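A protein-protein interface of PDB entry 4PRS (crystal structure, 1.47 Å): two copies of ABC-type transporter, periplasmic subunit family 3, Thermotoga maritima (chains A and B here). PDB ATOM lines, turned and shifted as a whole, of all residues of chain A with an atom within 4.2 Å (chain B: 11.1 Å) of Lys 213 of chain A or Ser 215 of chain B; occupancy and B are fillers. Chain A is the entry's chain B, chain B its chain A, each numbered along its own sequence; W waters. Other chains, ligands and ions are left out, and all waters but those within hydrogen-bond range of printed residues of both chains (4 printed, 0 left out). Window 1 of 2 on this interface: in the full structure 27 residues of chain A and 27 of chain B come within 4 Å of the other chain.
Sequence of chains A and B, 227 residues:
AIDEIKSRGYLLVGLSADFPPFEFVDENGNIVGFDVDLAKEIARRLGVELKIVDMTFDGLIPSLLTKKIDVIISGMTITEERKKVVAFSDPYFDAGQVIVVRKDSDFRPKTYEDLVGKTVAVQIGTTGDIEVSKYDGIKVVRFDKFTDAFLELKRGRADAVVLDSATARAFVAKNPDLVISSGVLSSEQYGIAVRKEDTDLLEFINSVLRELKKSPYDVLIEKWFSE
No residue of chain B comes within 4 Å of Pro 91 of chain A.
No residue of chain B comes within 4 Å of Leu 209 of chain A.
Of chain B, only Ser 215, Pro 216 and Tyr 217 come within 4 Å of Leu 212 of chain A.
Of the printed residues of chain B, Lys 213 of chain A touches Ser 215 (3.4 Å) and Tyr 217 (3.6 Å).
Ser 215 of chain A touches just these residues of chain B: Leu 212, Lys 213, Lys 214 and Ser 215.
Of the printed residues of chain A, Leu 212 of chain B touches Ser 215.
Printed residues of chain A within 4 Å of Ser 215 of chain B: Leu 212 (3.4 Å), Lys 213 (3.4 Å), Lys 214 (3.8 Å) and Ser 215 (3.9 Å).
Printed residues of chain A within 4 Å of Tyr 217 of chain B: Leu 212 and Lys 213.
The nearest printed residue of chain A that does not touch Tyr 217 of chain B is Leu 209 of chain A (5.8 Å).
Among the printed residues, pairs that only touch across the chains: Leu 212 of chain A with Ser 215 of chain B, Lys 213 of chain A with Ser 215 of chain B, Lys 213 of chain A with Tyr 217 of chain B, Lys 214 of chain A with Ser 215 of chain B, Lys 214 of chain A with Pro 216 of chain B, Ser 215 of chain A with Leu 212 of chain B, Ser 215 of chain A with Lys 213 of chain B, Ser 215 of chain A with Lys 214 of chain B and Ser 215 of chain A with Ser 215 of chain B.
Leu 212 of chain A touches Ser 215 of chain B, and with the chains exchanged Ser 215 of chain A touches Leu 212 of chain B.
Lys 213 of chain A touches Ser 215 of chain B, and with the chains exchanged Ser 215 of chain A touches Lys 213 of chain B.
Lys 214 of chain A touches Ser 215 of chain B, and with the chains exchanged Ser 215 of chain A touches Lys 214 of chain B.
Ser 215 of chain B touches its own counterpart, Ser 215 of chain A.
8 positions are printed for both chains.
Water W4 lies within hydrogen-bond range of the side-chain hydroxyl of Ser 215 of chain B (2.6 Å) and the backbone carbonyl oxygen of Lys 213 of chain A (2.8 Å).
Water W2 lies within hydrogen-bond range of OG of Ser 215 of chain A (2.6 Å), O of Lys 213 of chain B (3.1 Å) and OD1 of Asp 218 of chain A (3.5 Å).
Water W1 lies within hydrogen-bond range of NZ of Lys 213 of chain A (2.7 Å) and OH of Tyr 217 of chain B (3.3 Å).
Water W3 lies within hydrogen-bond range of the guanidinium group of Arg 210 of chain A (3.1 Å) and the backbone carbonyl oxygen of Ala 173 of chain B (3.4 Å).
NZ of Lys 214 of chain B lies within salt-bridge range of OE2 of Glu 222 of chain B (2.7 Å).
The side-chain hydroxyl (OG) of Ser 215 of chain B sits close to the backbone NH (N) of Tyr 217 of chain B (3.3 Å).
N of Ser 215 of chain B lies within hydrogen-bond range of OD2 of Asp 218 of chain B (2.9 Å).
The backbone NH (N) of Ser 215 of chain A lies within hydrogen-bond range of the side-chain carboxylate (OD2) of Asp 218 of chain A, at 2.9 Å.
Of the 9 printed residues of chain A, 4 touch a printed residue of chain B.
Hydrophobic or aromatic side chains of chain B within 4 Å of the printed part of chain A: Pro 216 and Tyr 217.
N of Tyr 217 of chain B sits at hydrogen-bond distance from O of Leu 212 of chain A.
The backbone nitrogen of Pro 216 of chain B sits close to the backbone carbonyl oxygen of Leu 212 of chain A.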
ATOM      1  N   PRO A  91      13.821   9.460  -7.323  1.00  0.00           N
ATOM      2  CA  PRO A  91      13.256  10.555  -6.538  1.00  0.00           C
ATOM      3  C   PRO A  91      12.426  10.084  -5.389  1.00  0.00           C
ATOM      4  O   PRO A  91      11.645   9.129  -5.471  1.00  0.00           O
ATOM      5  CB  PRO A  91      12.424  11.352  -7.551  1.00  0.00           C
ATOM      6  CG  PRO A  91      12.054  10.278  -8.604  1.00  0.00           C
ATOM      7  CD  PRO A  91      13.358   9.450  -8.746  1.00  0.00           C
ATOM      8  N   LEU A 209      13.944   2.452  -0.793  1.00  0.00           N
ATOM      9  CA  LEU A 209      12.868   3.420  -1.198  1.00  0.00           C
ATOM     10  C   LEU A 209      11.690   2.706  -1.887  1.00  0.00           C
ATOM     11  O   LEU A 209      10.531   3.033  -1.665  1.00  0.00           O
ATOM     12  CB  LEU A 209      13.424   4.461  -2.159  1.00  0.00           C
ATOM     13  CG  LEU A 209      14.489   5.439  -1.503  1.00  0.00           C
ATOM     14  CD1 LEU A 209      15.027   6.269  -2.666  1.00  0.00           C
ATOM     15  CD2 LEU A 209      13.809   6.334  -0.455  1.00  0.00           C
ATOM     16  N   ARG A 210      12.039   1.743  -2.755  1.00  0.00           N
ATOM     17  CA  ARG A 210      10.996   1.014  -3.508  1.00  0.00           C
ATOM     18  C   ARG A 210      10.134   0.252  -2.562  1.00  0.00           C
ATOM     19  O   ARG A 210       8.890   0.214  -2.719  1.00  0.00           O
ATOM     20  CB  ARG A 210      11.611   0.110  -4.640  1.00  0.00           C
ATOM     21  CG  ARG A 210      12.173   0.981  -5.765  1.00  0.00           C
ATOM     22  CD  ARG A 210      13.216   0.378  -6.623  1.00  0.00           C
ATOM     23  NE  ARG A 210      13.911   1.322  -7.496  1.00  0.00           N
ATOM     24  CZ  ARG A 210      14.874   0.988  -8.385  1.00  0.00           C
ATOM     25  NH1 ARG A 210      15.248  -0.295  -8.544  1.00  0.00           N
ATOM     26  NH2 ARG A 210      15.472   1.953  -9.112  1.00  0.00           N
ATOM     27  N   GLU A 211      10.755  -0.420  -1.582  1.00  0.00           N
ATOM     28  CA  GLU A 211       9.957  -1.162  -0.626  1.00  0.00           C
ATOM     29  C   GLU A 211       9.077  -0.209   0.235  1.00  0.00           C
ATOM     30  O   GLU A 211       7.861  -0.504   0.490  1.00  0.00           O
ATOM     31  CB  GLU A 211      10.812  -2.138   0.185  1.00  0.00           C
ATOM     32  CG  GLU A 211      10.080  -2.828   1.292  1.00  0.00           C
ATOM     33  CD  GLU A 211       9.307  -4.066   0.852  1.00  0.00           C
ATOM     34  OE1 GLU A 211       9.356  -4.473  -0.354  1.00  0.00           O
ATOM     35  OE2 GLU A 211       8.622  -4.635   1.740  1.00  0.00           O
ATOM     36  N   LEU A 212       9.611   0.928   0.663  1.00  0.00           N
ATOM     37  CA  LEU A 212       8.782   1.883   1.424  1.00  0.00           C
ATOM     38  C   LEU A 212       7.569   2.354   0.646  1.00  0.00           C
ATOM     39  O   LEU A 212       6.502   2.610   1.235  1.00  0.00           O
ATOM     40  CB  LEU A 212       9.622   3.102   1.884  1.00  0.00           C
ATOM     41  CG  LEU A 212      10.603   2.829   3.017  1.00  0.00           C
ATOM     42  CD1 LEU A 212      11.500   4.117   3.128  1.00  0.00           C
ATOM     43  CD2 LEU A 212       9.910   2.542   4.320  1.00  0.00           C
ATOM     44  N   LYS A 213       7.712   2.491  -0.668  1.00  0.00           N
ATOM     45  CA  LYS A 213       6.606   2.998  -1.507  1.00  0.00           C
ATOM     46  C   LYS A 213       5.594   1.916  -1.893  1.00  0.00           C
ATOM     47  O   LYS A 213       4.590   2.256  -2.504  1.00  0.00           O
ATOM     48  CB  LYS A 213       7.178   3.664  -2.756  1.00  0.00           C
ATOM     49  CG  LYS A 213       7.827   5.037  -2.447  1.00  0.00           C
ATOM     50  CD  LYS A 213       7.040   6.194  -3.060  1.00  0.00           C
ATOM     51  CE  LYS A 213       7.820   7.491  -2.939  1.00  0.00           C
ATOM     52  NZ  LYS A 213       8.539   7.951  -4.211  1.00  0.00           N
ATOM     53  N   LYS A 214       5.825   0.656  -1.516  1.00  0.00           N
ATOM     54  CA  LYS A 214       4.924  -0.421  -1.948  1.00  0.00           C
ATOM     55  C   LYS A 214       3.731  -0.553  -1.007  1.00  0.00           C
ATOM     56  O   LYS A 214       3.898  -0.822   0.205  1.00  0.00           O
ATOM     57  CB  LYS A 214       5.707  -1.745  -2.034  1.00  0.00           C
ATOM     58  CG  LYS A 214       6.507  -1.720  -3.343  1.00  0.00           C
ATOM     59  CD  LYS A 214       6.965  -3.110  -3.774  1.00  0.00           C
ATOM     60  CE  LYS A 214       7.795  -3.018  -5.077  1.00  0.00           C
ATOM     61  NZ  LYS A 214       8.759  -4.121  -5.291  1.00  0.00           N
ATOM     62  N   SER A 215       2.550  -0.358  -1.561  1.00  0.00           N
ATOM     63  CA  SER A 215       1.345  -0.512  -0.712  1.00  0.00           C
ATOM     64  C   SER A 215       0.798  -1.958  -0.909  1.00  0.00           C
ATOM     65  O   SER A 215       1.189  -2.694  -1.860  1.00  0.00           O
ATOM     66  CB  SER A 215       0.267   0.478  -1.216  1.00  0.00           C
ATOM     67  OG  SER A 215      -0.086   0.080  -2.570  1.00  0.00           O
ATOM     68  N   ASP A 218      -0.269  -2.317  -4.467  1.00  0.00           N
ATOM     69  CA  ASP A 218       0.801  -2.586  -5.356  1.00  0.00           C
ATOM     70  C   ASP A 218       1.188  -4.061  -5.341  1.00  0.00           C
ATOM     71  O   ASP A 218       1.503  -4.642  -6.392  1.00  0.00           O
ATOM     72  CB  ASP A 218       2.057  -1.761  -4.942  1.00  0.00           C
ATOM     73  CG  ASP A 218       1.837  -0.276  -5.110  1.00  0.00           C
ATOM     74  OD1 ASP A 218       1.062   0.217  -6.007  1.00  0.00           O
ATOM     75  OD2 ASP A 218       2.529   0.442  -4.351  1.00  0.00           O
ATOM     76  N   ALA B 173       8.453   0.329 -14.638  1.00  0.00           N
ATOM     77  CA  ALA B 173       9.035   0.707 -13.349  1.00  0.00           C
ATOM     78  C   ALA B 173      10.368  -0.007 -12.995  1.00  0.00           C
ATOM     79  O   ALA B 173      11.197   0.550 -12.255  1.00  0.00           O
ATOM     80  CB  ALA B 173       7.949   0.565 -12.162  1.00  0.00           C
ATOM     81  N   VAL B 208     -11.768   0.947   2.796  1.00  0.00           N
ATOM     82  CA  VAL B 208     -10.863  -0.209   2.620  1.00  0.00           C
ATOM     83  C   VAL B 208      -9.950   0.035   1.429  1.00  0.00           C
ATOM     84  O   VAL B 208      -8.757  -0.258   1.523  1.00  0.00           O
ATOM     85  CB  VAL B 208     -11.681  -1.457   2.385  1.00  0.00           C
ATOM     86  CG1 VAL B 208     -10.735  -2.671   1.961  1.00  0.00           C
ATOM     87  CG2 VAL B 208     -12.485  -1.801   3.637  1.00  0.00           C
ATOM     88  N   LEU B 209     -10.476   0.566   0.301  1.00  0.00           N
ATOM     89  CA  LEU B 209      -9.602   0.886  -0.848  1.00  0.00           C
ATOM     90  C   LEU B 209      -8.482   1.881  -0.436  1.00  0.00           C
ATOM     91  O   LEU B 209      -7.340   1.709  -0.862  1.00  0.00           O
ATOM     92  CB  LEU B 209     -10.429   1.415  -2.065  1.00  0.00           C
ATOM     93  CG  LEU B 209     -11.429   0.384  -2.658  1.00  0.00           C
ATOM     94  CD1 LEU B 209     -12.260   1.105  -3.699  1.00  0.00           C
ATOM     95  CD2 LEU B 209     -10.651  -0.741  -3.278  1.00  0.00           C
ATOM     96  N   ARG B 210      -8.836   2.918   0.336  1.00  0.00           N
ATOM     97  CA  ARG B 210      -7.823   3.877   0.821  1.00  0.00           C
ATOM     98  C   ARG B 210      -6.756   3.170   1.613  1.00  0.00           C
ATOM     99  O   ARG B 210      -5.543   3.440   1.425  1.00  0.00           O
ATOM    100  CB  ARG B 210      -8.439   5.048   1.634  1.00  0.00           C
ATOM    101  CG  ARG B 210      -9.199   6.079   0.774  1.00  0.00           C
ATOM    102  CD  ARG B 210      -9.806   7.238   1.676  1.00  0.00           C
ATOM    103  NE  ARG B 210     -11.267   7.135   1.828  1.00  0.00           N
ATOM    104  CZ  ARG B 210     -11.920   6.958   2.981  1.00  0.00           C
ATOM    105  NH1 ARG B 210     -11.273   6.876   4.150  1.00  0.00           N
ATOM    106  NH2 ARG B 210     -13.247   6.861   2.965  1.00  0.00           N
ATOM    107  N   GLU B 211      -7.138   2.356   2.411  1.00  0.00           N
ATOM    108  CA  GLU B 211      -6.173   1.644   3.224  1.00  0.00           C
ATOM    109  C   GLU B 211      -5.266   0.786   2.322  1.00  0.00           C
ATOM    110  O   GLU B 211      -4.034   0.674   2.576  1.00  0.00           O
ATOM    111  CB  GLU B 211      -6.884   0.722   4.222  1.00  0.00           C
ATOM    112  N   LEU B 212      -5.840   0.033   1.439  1.00  0.00           N
ATOM    113  CA  LEU B 212      -5.036  -0.869   0.603  1.00  0.00           C
ATOM    114  C   LEU B 212      -4.004  -0.081  -0.157  1.00  0.00           C
ATOM    115  O   LEU B 212      -2.929  -0.568  -0.449  1.00  0.00           O
ATOM    116  CB  LEU B 212      -5.894  -1.656  -0.381  1.00  0.00           C
ATOM    117  CG  LEU B 212      -6.737  -2.754   0.310  1.00  0.00           C
ATOM    118  CD1 LEU B 212      -7.663  -3.325  -0.726  1.00  0.00           C
ATOM    119  CD2 LEU B 212      -5.774  -3.859   0.811  1.00  0.00           C
ATOM    120  N   LYS B 213      -4.350   1.146  -0.505  1.00  0.00           N
ATOM    121  CA  LYS B 213      -3.433   1.954  -1.342  1.00  0.00           C
ATOM    122  C   LYS B 213      -2.382   2.754  -0.550  1.00  0.00           C
ATOM    123  O   LYS B 213      -1.534   3.427  -1.174  1.00  0.00           O
ATOM    124  CB  LYS B 213      -4.219   2.857  -2.270  1.00  0.00           C
ATOM    125  CG  LYS B 213      -4.858   2.054  -3.380  1.00  0.00           C
ATOM    126  CD  LYS B 213      -5.633   3.044  -4.320  1.00  0.00           C
ATOM    127  CE  LYS B 213      -6.034   2.323  -5.671  1.00  0.00           C
ATOM    128  NZ  LYS B 213      -6.767   3.367  -6.534  1.00  0.00           N
ATOM    129  N   LYS B 214      -2.421   2.661   0.802  1.00  0.00           N
ATOM    130  CA  LYS B 214      -1.488   3.446   1.629  1.00  0.00           C
ATOM    131  C   LYS B 214      -0.190   2.605   1.806  1.00  0.00           C
ATOM    132  O   LYS B 214      -0.210   1.398   2.192  1.00  0.00           O
ATOM    133  CB  LYS B 214      -2.117   3.702   3.017  1.00  0.00           C
ATOM    134  CG  LYS B 214      -1.328   4.734   3.855  1.00  0.00           C
ATOM    135  CD  LYS B 214      -2.022   5.228   5.081  1.00  0.00           C
ATOM    136  CE  LYS B 214      -3.310   5.951   4.762  1.00  0.00           C
ATOM    137  NZ  LYS B 214      -3.713   6.757   6.043  1.00  0.00           N
ATOM    138  N   SER B 215       0.950   3.277   1.644  1.00  0.00           N
ATOM    139  CA  SER B 215       2.261   2.613   1.773  1.00  0.00           C
ATOM    140  C   SER B 215       2.980   3.107   3.043  1.00  0.00           C
ATOM    141  O   SER B 215       2.553   4.129   3.639  1.00  0.00           O
ATOM    142  CB  SER B 215       3.186   2.872   0.582  1.00  0.00           C
ATOM    143  OG  SER B 215       3.405   4.281   0.569  1.00  0.00           O
ATOM    144  N   PRO B 216       4.039   2.393   3.482  1.00  0.00           N
ATOM    145  CA  PRO B 216       4.818   2.923   4.602  1.00  0.00           C
ATOM    146  C   PRO B 216       5.362   4.327   4.289  1.00  0.00           C
ATOM    147  O   PRO B 216       5.508   5.125   5.209  1.00  0.00           O
ATOM    148  CB  PRO B 216       5.986   1.900   4.737  1.00  0.00           C
ATOM    149  CG  PRO B 216       5.284   0.637   4.332  1.00  0.00           C
ATOM    150  CD  PRO B 216       4.500   1.032   3.104  1.00  0.00           C
ATOM    151  N   TYR B 217       5.665   4.620   3.006  1.00  0.00           N
ATOM    152  CA  TYR B 217       6.130   5.980   2.620  1.00  0.00           C
ATOM    153  C   TYR B 217       5.014   6.993   2.977  1.00  0.00           C
ATOM    154  O   TYR B 217       5.295   8.080   3.518  1.00  0.00           O
ATOM    155  CB  TYR B 217       6.455   6.017   1.146  1.00  0.00           C
ATOM    156  CG  TYR B 217       6.788   7.390   0.669  1.00  0.00           C
ATOM    157  CD1 TYR B 217       8.130   7.826   0.660  1.00  0.00           C
ATOM    158  CD2 TYR B 217       5.792   8.230   0.169  1.00  0.00           C
ATOM    159  CE1 TYR B 217       8.467   9.116   0.238  1.00  0.00           C
ATOM    160  CE2 TYR B 217       6.121   9.505  -0.305  1.00  0.00           C
ATOM    161  CZ  TYR B 217       7.455   9.940  -0.265  1.00  0.00           C
ATOM    162  OH  TYR B 217       7.781  11.209  -0.702  1.00  0.00           O
ATOM    163  N   ASP B 218       3.740   6.668   2.633  1.00  0.00           N
ATOM    164  CA  ASP B 218       2.602   7.554   2.956  1.00  0.00           C
ATOM    165  C   ASP B 218       2.524   7.780   4.460  1.00  0.00           C
ATOM    166  O   ASP B 218       2.236   8.909   4.929  1.00  0.00           O
ATOM    167  CB  ASP B 218       1.275   6.938   2.463  1.00  0.00           C
ATOM    168  CG  ASP B 218       1.216   6.864   0.979  1.00  0.00           C
ATOM    169  OD1 ASP B 218       1.773   7.773   0.306  1.00  0.00           O
ATOM    170  OD2 ASP B 218       0.611   5.902   0.444  1.00  0.00           O
ATOM    171  N   VAL B 219       2.770   6.755   5.256  1.00  0.00           N
ATOM    172  CA  VAL B 219       2.739   6.886   6.713  1.00  0.00           C
ATOM    173  C   VAL B 219       3.857   7.840   7.208  1.00  0.00           C
ATOM    174  O   VAL B 219       3.624   8.623   8.116  1.00  0.00           O
ATOM    175  CB  VAL B 219       2.778   5.476   7.412  1.00  0.00           C
ATOM    176  CG1 VAL B 219       2.969   5.583   8.926  1.00  0.00           C
ATOM    177  CG2 VAL B 219       1.483   4.628   7.064  1.00  0.00           C
ATOM    178  N   LEU B 220       5.029   7.783   6.568  1.00  0.00           N
ATOM    179  CA  LEU B 220       6.124   8.650   6.894  1.00  0.00           C
ATOM    180  C   LEU B 220       5.765  10.065   6.579  1.00  0.00           C
ATOM    181  O   LEU B 220       6.106  10.984   7.328  1.00  0.00           O
ATOM    182  CB  LEU B 220       7.419   8.174   6.189  1.00  0.00           C
ATOM    183  CG  LEU B 220       8.622   9.013   6.504  1.00  0.00           C
ATOM    184  CD1 LEU B 220       9.061   8.760   8.013  1.00  0.00           C
ATOM    185  CD2 LEU B 220       9.731   8.565   5.538  1.00  0.00           C
ATOM    186  N   ILE B 221       5.166  10.290   5.416  1.00  0.00           N
ATOM    187  CA  ILE B 221       4.681  11.666   5.127  1.00  0.00           C
ATOM    188  C   ILE B 221       3.672  12.135   6.225  1.00  0.00           C
ATOM    189  O   ILE B 221       3.749  13.280   6.640  1.00  0.00           O
ATOM    190  CB  ILE B 221       4.002  11.656   3.716  1.00  0.00           C
ATOM    191  CG1 ILE B 221       5.034  11.389   2.597  1.00  0.00           C
ATOM    192  CG2 ILE B 221       3.207  12.994   3.460  1.00  0.00           C
ATOM    193  CD1 ILE B 221       5.955  12.598   2.314  1.00  0.00           C
ATOM    194  N   GLU B 222       2.707  11.273   6.632  1.00  0.00           N
ATOM    195  CA  GLU B 222       1.802  11.625   7.682  1.00  0.00           C
ATOM    196  C   GLU B 222       2.518  11.975   8.978  1.00  0.00           C
ATOM    197  O   GLU B 222       2.139  12.968   9.698  1.00  0.00           O
ATOM    198  CB  GLU B 222       0.785  10.534   7.966  1.00  0.00           C
ATOM    199  CG  GLU B 222      -0.172  10.323   6.782  1.00  0.00           C
ATOM    200  CD  GLU B 222      -1.095   9.111   6.980  1.00  0.00           C
ATOM    201  OE1 GLU B 222      -1.036   8.450   8.085  1.00  0.00           O
ATOM    202  OE2 GLU B 222      -1.855   8.766   6.019  1.00  0.00           O
ATOM    203  N   LYS B 223       3.606  11.276   9.230  1.00  0.00           N
ATOM    204  CA  LYS B 223       4.356  11.585  10.477  1.00  0.00           C
ATOM    205  C   LYS B 223       4.939  12.975  10.493  1.00  0.00           C
ATOM    206  O   LYS B 223       4.879  13.671  11.537  1.00  0.00           O
ATOM    207  CB  LYS B 223       5.481  10.576  10.621  1.00  0.00           C
ATOM    208  CG  LYS B 223       6.300  10.777  11.908  1.00  0.00           C
ATOM    209  CD  LYS B 223       7.388   9.684  12.082  1.00  0.00           C
ATOM    210  CE  LYS B 223       8.352  10.015  13.258  1.00  0.00           C
ATOM    211  NZ  LYS B 223       9.453   9.017  13.429  1.00  0.00           N
HETATM  212  O   HOH W   1       8.249  10.672  -3.966  1.00  0.00           O
HETATM  213  O   HOH W   2      -0.888   2.188  -3.913  1.00  0.00           O
HETATM  214  O   HOH W   3      12.724  -1.414  -9.903  1.00  0.00           O
HETATM  215  O   HOH W   4       3.572   4.858  -1.960  1.00  0.00           O
